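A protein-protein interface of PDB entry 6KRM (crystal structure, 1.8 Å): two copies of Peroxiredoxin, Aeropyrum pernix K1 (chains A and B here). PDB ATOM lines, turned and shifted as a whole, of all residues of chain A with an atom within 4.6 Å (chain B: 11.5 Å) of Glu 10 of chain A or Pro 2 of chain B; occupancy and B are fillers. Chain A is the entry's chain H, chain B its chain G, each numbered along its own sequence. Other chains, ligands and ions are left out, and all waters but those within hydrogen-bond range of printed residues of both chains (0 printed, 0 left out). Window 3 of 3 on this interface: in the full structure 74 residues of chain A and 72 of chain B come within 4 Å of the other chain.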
ATOM      1  N   SER A   4      33.529  19.631  -0.678  1.00  0.00           N
ATOM      2  CA  SER A   4      33.178  19.849  -2.095  1.00  0.00           C
ATOM      3  C   SER A   4      32.767  18.507  -2.712  1.00  0.00           C
ATOM      4  O   SER A   4      33.394  17.500  -2.389  1.00  0.00           O
ATOM      5  CB  SER A   4      34.323  20.506  -2.827  1.00  0.00           C
ATOM      6  OG  SER A   4      33.920  20.798  -4.163  1.00  0.00           O
ATOM      7  N   ILE A   5      31.727  18.482  -3.543  1.00  0.00           N
ATOM      8  CA  ILE A   5      31.397  17.277  -4.367  1.00  0.00           C
ATOM      9  C   ILE A   5      31.131  17.671  -5.815  1.00  0.00           C
ATOM     10  O   ILE A   5      30.710  18.782  -6.126  1.00  0.00           O
ATOM     11  CB  ILE A   5      30.198  16.493  -3.805  1.00  0.00           C
ATOM     12  CG1 ILE A   5      28.963  17.393  -3.609  1.00  0.00           C
ATOM     13  CG2 ILE A   5      30.614  15.728  -2.547  1.00  0.00           C
ATOM     14  CD1 ILE A   5      27.642  16.643  -3.659  1.00  0.00           C
ATOM     15  N   PRO A   6      31.341  16.725  -6.753  1.00  0.00           N
ATOM     16  CA  PRO A   6      30.872  16.899  -8.118  1.00  0.00           C
ATOM     17  C   PRO A   6      29.341  16.932  -8.033  1.00  0.00           C
ATOM     18  O   PRO A   6      28.780  16.497  -7.020  1.00  0.00           O
ATOM     19  CB  PRO A   6      31.428  15.723  -8.921  1.00  0.00           C
ATOM     20  CG  PRO A   6      32.117  14.819  -7.918  1.00  0.00           C
ATOM     21  CD  PRO A   6      31.971  15.417  -6.529  1.00  0.00           C
ATOM     22  N   LEU A   7      28.685  17.482  -9.050  1.00  0.00           N
ATOM     23  CA  LEU A   7      27.231  17.763  -8.977  1.00  0.00           C
ATOM     24  C   LEU A   7      26.491  17.049 -10.105  1.00  0.00           C
ATOM     25  O   LEU A   7      27.047  16.798 -11.165  1.00  0.00           O
ATOM     26  CB  LEU A   7      27.009  19.269  -9.057  1.00  0.00           C
ATOM     27  CG  LEU A   7      27.658  20.090  -7.941  1.00  0.00           C
ATOM     28  CD1 LEU A   7      27.475  21.576  -8.199  1.00  0.00           C
ATOM     29  CD2 LEU A   7      27.082  19.722  -6.588  1.00  0.00           C
ATOM     30  N   ILE A   8      25.224  16.763  -9.862  1.00  0.00           N
ATOM     31  CA  ILE A   8      24.355  16.196 -10.912  1.00  0.00           C
ATOM     32  C   ILE A   8      24.335  17.180 -12.082  1.00  0.00           C
ATOM     33  O   ILE A   8      24.220  18.408 -11.836  1.00  0.00           O
ATOM     34  CB  ILE A   8      22.946  15.943 -10.360  1.00  0.00           C
ATOM     35  CG1 ILE A   8      22.950  14.863  -9.283  1.00  0.00           C
ATOM     36  CG2 ILE A   8      22.006  15.638 -11.518  1.00  0.00           C
ATOM     37  CD1 ILE A   8      21.673  14.790  -8.540  1.00  0.00           C
ATOM     38  N   GLY A   9      24.473  16.658 -13.304  1.00  0.00           N
ATOM     39  CA  GLY A   9      24.468  17.439 -14.549  1.00  0.00           C
ATOM     40  C   GLY A   9      25.875  17.868 -14.963  1.00  0.00           C
ATOM     41  O   GLY A   9      26.039  18.319 -16.103  1.00  0.00           O
ATOM     42  N   GLU A  10      26.881  17.692 -14.116  1.00  0.00           N
ATOM     43  CA  GLU A  10      28.288  17.970 -14.472  1.00  0.00           C
ATOM     44  C   GLU A  10      28.879  16.706 -15.092  1.00  0.00           C
ATOM     45  O   GLU A  10      28.491  15.590 -14.716  1.00  0.00           O
ATOM     46  CB  GLU A  10      29.128  18.337 -13.252  1.00  0.00           C
ATOM     47  CG  GLU A  10      28.765  19.653 -12.585  1.00  0.00           C
ATOM     48  CD  GLU A  10      29.703  20.044 -11.450  1.00  0.00           C
ATOM     49  OE1 GLU A  10      30.442  19.168 -10.915  1.00  0.00           O
ATOM     50  OE2 GLU A  10      29.657  21.209 -11.047  1.00  0.00           O
ATOM     51  N   ARG A  11      29.805  16.877 -16.017  1.00  0.00           N
ATOM     52  CA  ARG A  11      30.697  15.776 -16.465  1.00  0.00           C
ATOM     53  C   ARG A  11      31.453  15.248 -15.245  1.00  0.00           C
ATOM     54  O   ARG A  11      31.885  16.049 -14.389  1.00  0.00           O
ATOM     55  CB  ARG A  11      31.669  16.220 -17.562  1.00  0.00           C
ATOM     56  CG  ARG A  11      32.227  15.048 -18.359  1.00  0.00           C
ATOM     57  CD  ARG A  11      32.769  15.485 -19.709  1.00  0.00           C
ATOM     58  NE  ARG A  11      33.402  14.432 -20.497  1.00  0.00           N
ATOM     59  CZ  ARG A  11      34.599  13.933 -20.247  1.00  0.00           C
ATOM     60  NH1 ARG A  11      35.266  14.357 -19.182  1.00  0.00           N
ATOM     61  NH2 ARG A  11      35.112  12.989 -21.036  1.00  0.00           N
ATOM     62  N   PHE A  12      31.574  13.930 -15.143  1.00  0.00           N
ATOM     63  CA  PHE A  12      32.408  13.264 -14.127  1.00  0.00           C
ATOM     64  C   PHE A  12      33.820  13.829 -14.247  1.00  0.00           C
ATOM     65  O   PHE A  12      34.308  14.023 -15.346  1.00  0.00           O
ATOM     66  CB  PHE A  12      32.400  11.763 -14.382  1.00  0.00           C
ATOM     67  CG  PHE A  12      33.092  11.032 -13.298  1.00  0.00           C
ATOM     68  CD1 PHE A  12      32.415  10.728 -12.124  1.00  0.00           C
ATOM     69  CD2 PHE A  12      34.433  10.722 -13.416  1.00  0.00           C
ATOM     70  CE1 PHE A  12      33.055  10.028 -11.120  1.00  0.00           C
ATOM     71  CE2 PHE A  12      35.080  10.081 -12.379  1.00  0.00           C
ATOM     72  CZ  PHE A  12      34.393   9.731 -11.255  1.00  0.00           C
ATOM     73  N   GLY A 135      29.075  10.630 -19.983  1.00  0.00           N
ATOM     74  CA  GLY A 135      29.994  10.931 -18.876  1.00  0.00           C
ATOM     75  C   GLY A 135      29.419  11.953 -17.910  1.00  0.00           C
ATOM     76  O   GLY A 135      30.205  12.533 -17.161  1.00  0.00           O
ATOM     77  N   VAL A 136      28.100  12.123 -17.882  1.00  0.00           N
ATOM     78  CA  VAL A 136      27.413  13.097 -17.001  1.00  0.00           C
ATOM     79  C   VAL A 136      26.949  12.370 -15.741  1.00  0.00           C
ATOM     80  O   VAL A 136      26.277  11.324 -15.811  1.00  0.00           O
ATOM     81  CB  VAL A 136      26.267  13.806 -17.754  1.00  0.00           C
ATOM     82  CG1 VAL A 136      25.466  14.734 -16.844  1.00  0.00           C
ATOM     83  CG2 VAL A 136      26.800  14.562 -18.982  1.00  0.00           C
ATOM     84  N   ILE A 137      27.207  12.974 -14.585  1.00  0.00           N
ATOM     85  CA  ILE A 137      26.700  12.475 -13.291  1.00  0.00           C
ATOM     86  C   ILE A 137      25.169  12.650 -13.250  1.00  0.00           C
ATOM     87  O   ILE A 137      24.665  13.747 -13.467  1.00  0.00           O
ATOM     88  CB  ILE A 137      27.402  13.203 -12.134  1.00  0.00           C
ATOM     89  CG1 ILE A 137      28.909  12.935 -12.106  1.00  0.00           C
ATOM     90  CG2 ILE A 137      26.763  12.837 -10.830  1.00  0.00           C
ATOM     91  CD1 ILE A 137      29.674  13.891 -11.204  1.00  0.00           C
ATOM     92  N   PRO B   2      32.564  20.463  -7.541  1.00  0.00           N
ATOM     93  CA  PRO B   2      32.080  21.826  -7.814  1.00  0.00           C
ATOM     94  C   PRO B   2      30.861  22.323  -7.026  1.00  0.00           C
ATOM     95  O   PRO B   2      30.381  23.374  -7.377  1.00  0.00           O
ATOM     96  CB  PRO B   2      31.792  21.740  -9.312  1.00  0.00           C
ATOM     97  CG  PRO B   2      33.037  21.024  -9.805  1.00  0.00           C
ATOM     98  CD  PRO B   2      33.646  20.393  -8.556  1.00  0.00           C
ATOM     99  N   GLY B   3      30.483  21.654  -5.934  1.00  0.00           N
ATOM    100  CA  GLY B   3      29.589  22.263  -4.925  1.00  0.00           C
ATOM    101  C   GLY B   3      29.875  21.784  -3.506  1.00  0.00           C
ATOM    102  O   GLY B   3      30.087  20.579  -3.311  1.00  0.00           O
ATOM    103  N   SER B   4      29.772  22.672  -2.516  1.00  0.00           N
ATOM    104  CA  SER B   4      29.955  22.311  -1.080  1.00  0.00           C
ATOM    105  C   SER B   4      28.686  21.607  -0.555  1.00  0.00           C
ATOM    106  O   SER B   4      27.572  22.069  -0.853  1.00  0.00           O
ATOM    107  CB  SER B   4      30.332  23.533  -0.272  1.00  0.00           C
ATOM    108  OG  SER B   4      30.619  23.188   1.075  1.00  0.00           O
ATOM    109  N   ILE B   5      28.839  20.508   0.185  1.00  0.00           N
ATOM    110  CA  ILE B   5      27.718  19.874   0.935  1.00  0.00           C
ATOM    111  C   ILE B   5      28.097  19.711   2.404  1.00  0.00           C
ATOM    112  O   ILE B   5      29.262  19.678   2.776  1.00  0.00           O
ATOM    113  CB  ILE B   5      27.300  18.531   0.292  1.00  0.00           C
ATOM    114  CG1 ILE B   5      28.460  17.539   0.192  1.00  0.00           C
ATOM    115  CG2 ILE B   5      26.656  18.770  -1.062  1.00  0.00           C
ATOM    116  CD1 ILE B   5      28.013  16.104  -0.003  1.00  0.00           C
ATOM    117  N   PRO B   6      27.106  19.611   3.313  1.00  0.00           N
ATOM    118  CA  PRO B   6      27.370  19.102   4.654  1.00  0.00           C
ATOM    119  C   PRO B   6      27.777  17.629   4.488  1.00  0.00           C
ATOM    120  O   PRO B   6      27.536  17.077   3.396  1.00  0.00           O
ATOM    121  CB  PRO B   6      26.035  19.186   5.412  1.00  0.00           C
ATOM    122  CG  PRO B   6      25.070  19.916   4.468  1.00  0.00           C
ATOM    123  CD  PRO B   6      25.677  19.891   3.076  1.00  0.00           C
ATOM    124  N   ALA B 110      19.162  26.232   0.193  1.00  0.00           N
ATOM    125  CA  ALA B 110      19.607  25.321  -0.895  1.00  0.00           C
ATOM    126  C   ALA B 110      21.136  25.441  -1.027  1.00  0.00           C
ATOM    127  O   ALA B 110      21.830  24.420  -1.026  1.00  0.00           O
ATOM    128  CB  ALA B 110      18.857  25.669  -2.163  1.00  0.00           C
ATOM    129  N   ARG B 111      21.686  26.657  -1.007  1.00  0.00           N
ATOM    130  CA  ARG B 111      23.159  26.837  -1.178  1.00  0.00           C
ATOM    131  C   ARG B 111      23.864  26.272   0.055  1.00  0.00           C
ATOM    132  O   ARG B 111      24.866  25.641  -0.095  1.00  0.00           O
ATOM    133  CB  ARG B 111      23.485  28.315  -1.415  1.00  0.00           C
ATOM    134  CG  ARG B 111      24.562  28.592  -2.450  1.00  0.00           C
ATOM    135  CD  ARG B 111      24.623  30.081  -2.798  1.00  0.00           C
ATOM    136  NE  ARG B 111      23.332  30.490  -3.337  1.00  0.00           N
ATOM    137  CZ  ARG B 111      22.450  31.316  -2.759  1.00  0.00           C
ATOM    138  NH1 ARG B 111      22.698  31.895  -1.591  1.00  0.00           N
ATOM    139  NH2 ARG B 111      21.304  31.565  -3.377  1.00  0.00           N
ATOM    140  N   LEU B 113      22.999  23.711   1.877  1.00  0.00           N
ATOM    141  CA  LEU B 113      22.922  22.235   1.883  1.00  0.00           C
ATOM    142  C   LEU B 113      23.459  21.649   0.569  1.00  0.00           C
ATOM    143  O   LEU B 113      23.384  20.422   0.430  1.00  0.00           O
ATOM    144  CB  LEU B 113      21.454  21.841   2.104  1.00  0.00           C
ATOM    145  CG  LEU B 113      20.833  22.339   3.422  1.00  0.00           C
ATOM    146  CD1 LEU B 113      19.405  21.825   3.597  1.00  0.00           C
ATOM    147  CD2 LEU B 113      21.668  21.915   4.611  1.00  0.00           C
ATOM    148  N   GLY B 114      23.923  22.480  -0.370  1.00  0.00           N
ATOM    149  CA  GLY B 114      24.506  21.984  -1.638  1.00  0.00           C
ATOM    150  C   GLY B 114      23.454  21.386  -2.555  1.00  0.00           C
ATOM    151  O   GLY B 114      23.732  20.348  -3.189  1.00  0.00           O
ATOM    152  N   LEU B 115      22.247  21.969  -2.580  1.00  0.00           N
ATOM    153  CA  LEU B 115      21.090  21.368  -3.299  1.00  0.00           C
ATOM    154  C   LEU B 115      20.920  21.989  -4.689  1.00  0.00           C
ATOM    155  O   LEU B 115      20.037  21.506  -5.456  1.00  0.00           O
ATOM    156  CB  LEU B 115      19.819  21.522  -2.477  1.00  0.00           C
ATOM    157  CG  LEU B 115      19.778  20.702  -1.194  1.00  0.00           C
ATOM    158  CD1 LEU B 115      18.560  21.055  -0.384  1.00  0.00           C
ATOM    159  CD2 LEU B 115      19.794  19.211  -1.500  1.00  0.00           C
ATOM    160  N   LEU B 116      21.730  22.982  -5.042  1.00  0.00           N
ATOM    161  CA  LEU B 116      21.750  23.533  -6.417  1.00  0.00           C
ATOM    162  C   LEU B 116      22.868  22.850  -7.198  1.00  0.00           C
ATOM    163  O   LEU B 116      24.052  23.148  -6.975  1.00  0.00           O
ATOM    164  CB  LEU B 116      21.980  25.041  -6.344  1.00  0.00           C
ATOM    165  CG  LEU B 116      20.790  26.000  -6.371  1.00  0.00           C
ATOM    166  CD1 LEU B 116      19.416  25.369  -6.411  1.00  0.00           C
ATOM    167  CD2 LEU B 116      20.919  27.011  -5.239  1.00  0.00           C
ATOM    168  N   HIS B 117      22.513  21.990  -8.136  1.00  0.00           N
ATOM    169  CA  HIS B 117      23.490  21.238  -8.958  1.00  0.00           C
ATOM    170  C   HIS B 117      23.452  21.839 -10.358  1.00  0.00           C
ATOM    171  O   HIS B 117      22.777  22.849 -10.530  1.00  0.00           O
ATOM    172  CB  HIS B 117      23.177  19.738  -8.896  1.00  0.00           C
ATOM    173  CG  HIS B 117      23.447  19.139  -7.552  1.00  0.00           C
ATOM    174  ND1 HIS B 117      23.945  17.861  -7.418  1.00  0.00           N
ATOM    175  CD2 HIS B 117      23.338  19.633  -6.291  1.00  0.00           C
ATOM    176  CE1 HIS B 117      24.085  17.577  -6.130  1.00  0.00           C
ATOM    177  NE2 HIS B 117      23.690  18.641  -5.420  1.00  0.00           N
ATOM    178  N   ALA B 118      24.116  21.212 -11.322  1.00  0.00           N
ATOM    179  CA  ALA B 118      24.343  21.799 -12.661  1.00  0.00           C
ATOM    180  C   ALA B 118      23.122  21.567 -13.540  1.00  0.00           C
ATOM    181  O   ALA B 118      22.992  22.230 -14.559  1.00  0.00           O
ATOM    182  CB  ALA B 118      25.606  21.218 -13.248  1.00  0.00           C
ATOM    183  N   GLU B 119      22.226  20.667 -13.159  1.00  0.00           N
ATOM    184  CA  GLU B 119      21.036  20.308 -13.960  1.00  0.00           C
ATOM    185  C   GLU B 119      20.045  21.487 -13.997  1.00  0.00           C
ATOM    186  O   GLU B 119      19.382  21.673 -15.015  1.00  0.00           O
ATOM    187  CB  GLU B 119      20.471  19.001 -13.395  1.00  0.00           C
ATOM    188  CG  GLU B 119      19.368  18.412 -14.224  1.00  0.00           C
ATOM    189  CD  GLU B 119      18.826  17.075 -13.736  1.00  0.00           C
ATOM    190  OE1 GLU B 119      18.581  16.911 -12.501  1.00  0.00           O
ATOM    191  OE2 GLU B 119      18.532  16.260 -14.613  1.00  0.00           O
ATOM    192  N   SER B 120      20.000  22.316 -12.970  1.00  0.00           N
ATOM    193  CA  SER B 120      19.145  23.525 -12.935  1.00  0.00           C
ATOM    194  C   SER B 120      19.857  24.598 -12.140  1.00  0.00           C
ATOM    195  O   SER B 120      20.247  24.321 -11.042  1.00  0.00           O
ATOM    196  CB  SER B 120      17.794  23.209 -12.337  1.00  0.00           C
ATOM    197  OG  SER B 120      16.980  24.373 -12.261  1.00  0.00           O
ATOM    198  N   ALA B 121      19.989  25.801 -12.679  1.00  0.00           N
ATOM    199  CA  ALA B 121      20.550  26.943 -11.931  1.00  0.00           C
ATOM    200  C   ALA B 121      19.489  27.464 -10.959  1.00  0.00           C
ATOM    201  O   ALA B 121      19.884  28.168 -10.040  1.00  0.00           O
ATOM    202  CB  ALA B 121      20.998  28.039 -12.888  1.00  0.00           C
ATOM    203  N   VAL B 125      17.817  20.119  -6.674  1.00  0.00           N
ATOM    204  CA  VAL B 125      17.659  18.670  -7.008  1.00  0.00           C
ATOM    205  C   VAL B 125      16.745  18.014  -5.960  1.00  0.00           C
ATOM    206  O   VAL B 125      16.100  18.749  -5.143  1.00  0.00           O
ATOM    207  CB  VAL B 125      19.024  17.973  -7.114  1.00  0.00           C
ATOM    208  CG1 VAL B 125      19.825  18.530  -8.286  1.00  0.00           C
ATOM    209  CG2 VAL B 125      19.790  18.036  -5.829  1.00  0.00           C
ATOM    210  N   TYR B 142      21.062  12.153  -3.397  1.00  0.00           N
ATOM    211  CA  TYR B 142      20.866  13.209  -4.401  1.00  0.00           C
ATOM    212  C   TYR B 142      20.307  12.566  -5.651  1.00  0.00           C
ATOM    213  O   TYR B 142      21.060  12.002  -6.454  1.00  0.00           O
ATOM    214  CB  TYR B 142      22.151  13.986  -4.666  1.00  0.00           C
ATOM    215  CG  TYR B 142      22.668  14.740  -3.460  1.00  0.00           C
ATOM    216  CD1 TYR B 142      22.241  16.031  -3.170  1.00  0.00           C
ATOM    217  CD2 TYR B 142      23.590  14.164  -2.602  1.00  0.00           C
ATOM    218  CE1 TYR B 142      22.699  16.725  -2.057  1.00  0.00           C
ATOM    219  CE2 TYR B 142      24.054  14.846  -1.483  1.00  0.00           C
ATOM    220  CZ  TYR B 142      23.634  16.139  -1.228  1.00  0.00           C
ATOM    221  OH  TYR B 142      24.052  16.803  -0.092  1.00  0.00           O
ATOM    222  N   PRO B 144      17.871  13.249  -9.146  1.00  0.00           N
ATOM    223  CA  PRO B 144      17.765  14.345 -10.090  1.00  0.00           C
ATOM    224  C   PRO B 144      16.312  14.779 -10.353  1.00  0.00           C
ATOM    225  O   PRO B 144      15.384  14.118  -9.888  1.00  0.00           O
ATOM    226  CB  PRO B 144      18.345  13.671 -11.340  1.00  0.00           C
ATOM    227  CG  PRO B 144      17.828  12.263 -11.266  1.00  0.00           C
ATOM    228  CD  PRO B 144      17.794  11.937  -9.786  1.00  0.00           C
ATOM    229  N   MET B 145      16.120  15.783 -11.204  1.00  0.00           N
ATOM    230  CA  MET B 145      14.750  16.318 -11.512  1.00  0.00           C
ATOM    231  C   MET B 145      13.853  15.211 -12.105  1.00  0.00           C
ATOM    232  O   MET B 145      12.617  15.193 -11.827  1.00  0.00           O
ATOM    233  CB  MET B 145      14.819  17.431 -12.559  1.00  0.00           C
ATOM    234  CG  MET B 145      15.770  18.516 -12.262  1.00  0.00           C
ATOM    235  SD  MET B 145      15.652  19.020 -10.520  1.00  0.00           S
ATOM    236  CE  MET B 145      16.402  20.644 -10.572  1.00  0.00           C
ATOM    237  N   GLU B 146      14.419  14.371 -12.957  1.00  0.00           N
ATOM    238  CA  GLU B 146      13.658  13.473 -13.853  1.00  0.00           C
ATOM    239  C   GLU B 146      13.290  12.143 -13.170  1.00  0.00           C
ATOM    240  O   GLU B 146      12.620  11.320 -13.821  1.00  0.00           O
ATOM    241  CB  GLU B 146      14.416  13.235 -15.158  1.00  0.00           C
ATOM    242  CG  GLU B 146      15.746  12.493 -15.014  1.00  0.00           C
ATOM    243  CD  GLU B 146      16.981  13.348 -14.781  1.00  0.00           C
ATOM    244  OE1 GLU B 146      18.089  12.853 -15.106  1.00  0.00           O
ATOM    245  OE2 GLU B 146      16.859  14.500 -14.265  1.00  0.00           O
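The backbone NH of Glu 119 of chain B is in hydrogen-bond range of the backbone carbonyl oxygen of Ile 8 of chain A (3.3 Å).
The backbone carbonyl oxygen (O) of Ile 8 of chain A lies within hydrogen-bond range of the backbone NH (N) of Ala 118 of chain B, at 2.9 Å.
A ring nitrogen (ND1) of His 117 of chain B sits at hydrogen-bond distance from the backbone NH of Ile 8 of chain A (3.0 Å).
The backbone carbonyl oxygen of Gly 3 of chain B sits at hydrogen-bond distance from the backbone NH of Ile 5 of chain A, 2.7 Å away.
The backbone carbonyl oxygen of Ile 5 of chain A sits close to the backbone nitrogen of Pro 2 of chain B (2.9 Å).
OE2 of Glu 146 of chain B lies close to OE2 of Glu 119 of chain B (2.5 Å).
The backbone NH of Leu 7 of chain A is in hydrogen-bond range of the side-chain carboxylate of Glu 10 of chain A (3.1 Å).
NE2 of His 117 of chain B sits at hydrogen-bond distance from O of Gly 114 of chain B (2.8 Å).
The side-chain carboxylate of Glu 119 of chain B is in hydrogen-bond range of the backbone NH of Met 145 of chain B.
O of Glu 10 of chain A is in hydrogen-bond range of N of Ile 137 of chain A.
The backbone NH (N) of Gly 9 of chain A sits at hydrogen-bond distance from the backbone carbonyl oxygen (O) of Ile 137 of chain A (2.9 Å).
Among the printed residues, merely in contact across the chains: Ser 4 of chain A with Pro 2 of chain B (3.7 Å), Ser 4 of chain A with Gly 3 of chain B (3.4 Å), Ile 5 of chain A with Ile 5 of chain B (3.5 Å), Pro 6 of chain A with Pro 2 of chain B (3.99 Å), Leu 7 of chain A with Pro 2 of chain B (3.5 Å), Leu 7 of chain A with Gly 3 of chain B (3.8 Å), Leu 7 of chain A with Leu 116 of chain B (3.96 Å), Leu 7 of chain A with His 117 of chain B (3.6 Å), Ile 8 of chain A with Tyr 142 of chain B (3.5 Å), Gly 9 of chain A with Ala 118 of chain B (3.8 Å), Glu 10 of chain A with Pro 2 of chain B (2.8 Å) and Glu 10 of chain A with Ala 118 of chain B (3.6 Å).
Glu 10 of chain A touches just these residues of chain B: Pro 2 and Ala 118.
No residue of chain B comes within 4 Å of Gly 135 of chain A.
No residue of chain B comes within 4 Å of Ile 137 of chain A.
Of the printed residues of chain A, Glu 119 of chain B touches Ile 8.
Of the printed residues of chain A, Leu 116 of chain B touches Leu 7 (3.96 Å).
Ser 4 of chain B touches none of the printed residues of chain A.
The nearest residue of chain B that does not touch Glu 10 of chain A is Gly 3 of chain B (5.2 Å).
Along chain B the printed residues that touch a printed residue of chain A span positions 2 to 142.
Among the printed residues, 17 pairs touch across the chains.
Ile 5 of chain B touches its own counterpart, Ile 5 of chain A.
3 positions are printed for both chains.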
